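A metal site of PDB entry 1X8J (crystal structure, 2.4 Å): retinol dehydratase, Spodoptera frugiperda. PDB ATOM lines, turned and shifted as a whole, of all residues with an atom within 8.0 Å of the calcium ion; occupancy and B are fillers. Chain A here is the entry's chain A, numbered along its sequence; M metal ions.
The backbone NH of Asn 121 is in hydrogen-bond range of the side-chain hydroxyl of Tyr 135 (3.4 Å).
Of the 10 residues printed, 3 come within 4 Å of the calcium ion. Along chain A the residues within 4 Å of the calcium ion span positions 118 to 122. The nearest printed residue that does not touch the calcium ion is Glu 119 (5.0 Å).
The calcium ion is bound by the side-chain carboxylate of Asp 122 (2.5 Å), the side-chain amide oxygen of Asn 121 (2.5 Å) and the backbone carbonyl oxygen of Glu 118 (2.8 Å). The calcium ion has three donor atoms within binding distance.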
ATOM      1  N   LYS A 116     -10.700 -10.197 -14.668  1.00  0.00           N
ATOM      2  CA  LYS A 116     -10.229  -9.589 -13.431  1.00  0.00           C
ATOM      3  C   LYS A 116      -9.470 -10.569 -12.552  1.00  0.00           C
ATOM      4  O   LYS A 116      -9.418 -10.386 -11.333  1.00  0.00           O
ATOM      5  CB  LYS A 116     -11.402  -9.027 -12.639  1.00  0.00           C
ATOM      6  CG  LYS A 116     -12.369  -8.142 -13.420  1.00  0.00           C
ATOM      7  CD  LYS A 116     -13.346  -7.469 -12.459  1.00  0.00           C
ATOM      8  CE  LYS A 116     -14.337  -6.576 -13.185  1.00  0.00           C
ATOM      9  NZ  LYS A 116     -15.293  -7.404 -13.964  1.00  0.00           N
ATOM     10  N   GLN A 117      -8.877 -11.597 -13.157  1.00  0.00           N
ATOM     11  CA  GLN A 117      -8.150 -12.603 -12.391  1.00  0.00           C
ATOM     12  C   GLN A 117      -7.291 -12.015 -11.270  1.00  0.00           C
ATOM     13  O   GLN A 117      -7.375 -12.468 -10.127  1.00  0.00           O
ATOM     14  CB  GLN A 117      -7.269 -13.447 -13.302  1.00  0.00           C
ATOM     15  CG  GLN A 117      -6.627 -14.642 -12.577  1.00  0.00           C
ATOM     16  CD  GLN A 117      -5.695 -15.469 -13.464  1.00  0.00           C
ATOM     17  OE1 GLN A 117      -6.056 -15.850 -14.580  1.00  0.00           O
ATOM     18  NE2 GLN A 117      -4.495 -15.747 -12.963  1.00  0.00           N
ATOM     19  N   GLU A 118      -6.481 -11.016 -11.590  1.00  0.00           N
ATOM     20  CA  GLU A 118      -5.600 -10.403 -10.598  1.00  0.00           C
ATOM     21  C   GLU A 118      -6.340  -9.806  -9.400  1.00  0.00           C
ATOM     22  O   GLU A 118      -5.799  -9.760  -8.297  1.00  0.00           O
ATOM     23  CB  GLU A 118      -4.747  -9.277 -11.211  1.00  0.00           C
ATOM     24  CG  GLU A 118      -3.767  -9.678 -12.302  1.00  0.00           C
ATOM     25  CD  GLU A 118      -4.427  -9.886 -13.655  1.00  0.00           C
ATOM     26  OE1 GLU A 118      -3.677  -9.909 -14.666  1.00  0.00           O
ATOM     27  OE2 GLU A 118      -5.665 -10.033 -13.709  1.00  0.00           O
ATOM     28  N   GLU A 119      -7.566  -9.350  -9.632  1.00  0.00           N
ATOM     29  CA  GLU A 119      -8.360  -8.711  -8.586  1.00  0.00           C
ATOM     30  C   GLU A 119      -8.951  -9.586  -7.487  1.00  0.00           C
ATOM     31  O   GLU A 119      -9.216  -9.091  -6.388  1.00  0.00           O
ATOM     32  CB  GLU A 119      -9.501  -7.906  -9.239  1.00  0.00           C
ATOM     33  CG  GLU A 119      -9.042  -6.662  -9.958  1.00  0.00           C
ATOM     34  CD  GLU A 119     -10.114  -6.089 -10.866  1.00  0.00           C
ATOM     35  OE1 GLU A 119     -11.252  -5.890 -10.399  1.00  0.00           O
ATOM     36  OE2 GLU A 119      -9.816  -5.857 -12.056  1.00  0.00           O
ATOM     37  N   TYR A 120      -9.145 -10.875  -7.752  1.00  0.00           N
ATOM     38  CA  TYR A 120      -9.756 -11.746  -6.763  1.00  0.00           C
ATOM     39  C   TYR A 120      -8.987 -12.055  -5.481  1.00  0.00           C
ATOM     40  O   TYR A 120      -9.591 -12.109  -4.405  1.00  0.00           O
ATOM     41  CB  TYR A 120     -10.192 -13.042  -7.411  1.00  0.00           C
ATOM     42  CG  TYR A 120     -11.327 -12.812  -8.361  1.00  0.00           C
ATOM     43  CD1 TYR A 120     -11.082 -12.601  -9.722  1.00  0.00           C
ATOM     44  CD2 TYR A 120     -12.645 -12.776  -7.911  1.00  0.00           C
ATOM     45  CE1 TYR A 120     -12.116 -12.352 -10.611  1.00  0.00           C
ATOM     46  CE2 TYR A 120     -13.692 -12.519  -8.784  1.00  0.00           C
ATOM     47  CZ  TYR A 120     -13.420 -12.307 -10.137  1.00  0.00           C
ATOM     48  OH  TYR A 120     -14.457 -12.072 -11.017  1.00  0.00           O
ATOM     49  N   ASN A 121      -7.677 -12.250  -5.575  1.00  0.00           N
ATOM     50  CA  ASN A 121      -6.901 -12.568  -4.394  1.00  0.00           C
ATOM     51  C   ASN A 121      -6.782 -11.372  -3.450  1.00  0.00           C
ATOM     52  O   ASN A 121      -6.428 -11.528  -2.281  1.00  0.00           O
ATOM     53  CB  ASN A 121      -5.512 -13.089  -4.791  1.00  0.00           C
ATOM     54  CG  ASN A 121      -4.580 -11.977  -5.244  1.00  0.00           C
ATOM     55  OD1 ASN A 121      -4.956 -11.102  -6.030  1.00  0.00           O
ATOM     56  ND2 ASN A 121      -3.344 -12.013  -4.749  1.00  0.00           N
ATOM     57  N   ASP A 122      -7.107 -10.189  -3.948  1.00  0.00           N
ATOM     58  CA  ASP A 122      -7.013  -8.977  -3.147  1.00  0.00           C
ATOM     59  C   ASP A 122      -8.118  -8.850  -2.096  1.00  0.00           C
ATOM     60  O   ASP A 122      -8.084  -7.944  -1.275  1.00  0.00           O
ATOM     61  CB  ASP A 122      -7.046  -7.741  -4.051  1.00  0.00           C
ATOM     62  CG  ASP A 122      -6.026  -7.816  -5.169  1.00  0.00           C
ATOM     63  OD1 ASP A 122      -4.955  -8.448  -4.989  1.00  0.00           O
ATOM     64  OD2 ASP A 122      -6.283  -7.237  -6.247  1.00  0.00           O
ATOM     65  N   ILE A 123      -9.094  -9.745  -2.109  1.00  0.00           N
ATOM     66  CA  ILE A 123     -10.164  -9.690  -1.119  1.00  0.00           C
ATOM     67  C   ILE A 123      -9.774 -10.515   0.097  1.00  0.00           C
ATOM     68  O   ILE A 123     -10.471 -10.512   1.103  1.00  0.00           O
ATOM     69  CB  ILE A 123     -11.501 -10.226  -1.692  1.00  0.00           C
ATOM     70  CG1 ILE A 123     -11.391 -11.718  -1.958  1.00  0.00           C
ATOM     71  CG2 ILE A 123     -11.864  -9.480  -2.961  1.00  0.00           C
ATOM     72  CD1 ILE A 123     -12.630 -12.322  -2.554  1.00  0.00           C
ATOM     73  N   PRO A 127      -3.347 -12.997   1.054  1.00  0.00           N
ATOM     74  CA  PRO A 127      -3.162 -13.615  -0.262  1.00  0.00           C
ATOM     75  C   PRO A 127      -1.949 -14.534  -0.326  1.00  0.00           C
ATOM     76  O   PRO A 127      -1.966 -15.575  -0.983  1.00  0.00           O
ATOM     77  CB  PRO A 127      -3.001 -12.409  -1.192  1.00  0.00           C
ATOM     78  CG  PRO A 127      -3.782 -11.342  -0.507  1.00  0.00           C
ATOM     79  CD  PRO A 127      -3.418 -11.531   0.936  1.00  0.00           C
ATOM     80  N   TYR A 135      -5.340 -23.074  -5.941  1.00  0.00           N
ATOM     81  CA  TYR A 135      -6.110 -21.846  -6.152  1.00  0.00           C
ATOM     82  C   TYR A 135      -6.290 -21.575  -7.658  1.00  0.00           C
ATOM     83  O   TYR A 135      -7.397 -21.358  -8.141  1.00  0.00           O
ATOM     84  CB  TYR A 135      -5.399 -20.661  -5.495  1.00  0.00           C
ATOM     85  CG  TYR A 135      -6.084 -19.330  -5.663  1.00  0.00           C
ATOM     86  CD1 TYR A 135      -7.220 -18.995  -4.917  1.00  0.00           C
ATOM     87  CD2 TYR A 135      -5.597 -18.381  -6.564  1.00  0.00           C
ATOM     88  CE1 TYR A 135      -7.837 -17.752  -5.074  1.00  0.00           C
ATOM     89  CE2 TYR A 135      -6.208 -17.146  -6.719  1.00  0.00           C
ATOM     90  CZ  TYR A 135      -7.320 -16.831  -5.977  1.00  0.00           C
ATOM     91  OH  TYR A 135      -7.894 -15.588  -6.131  1.00  0.00           O
HETATM   92 CA    CA M   1      -3.474  -9.219  -6.811  1.00  0.00          CA
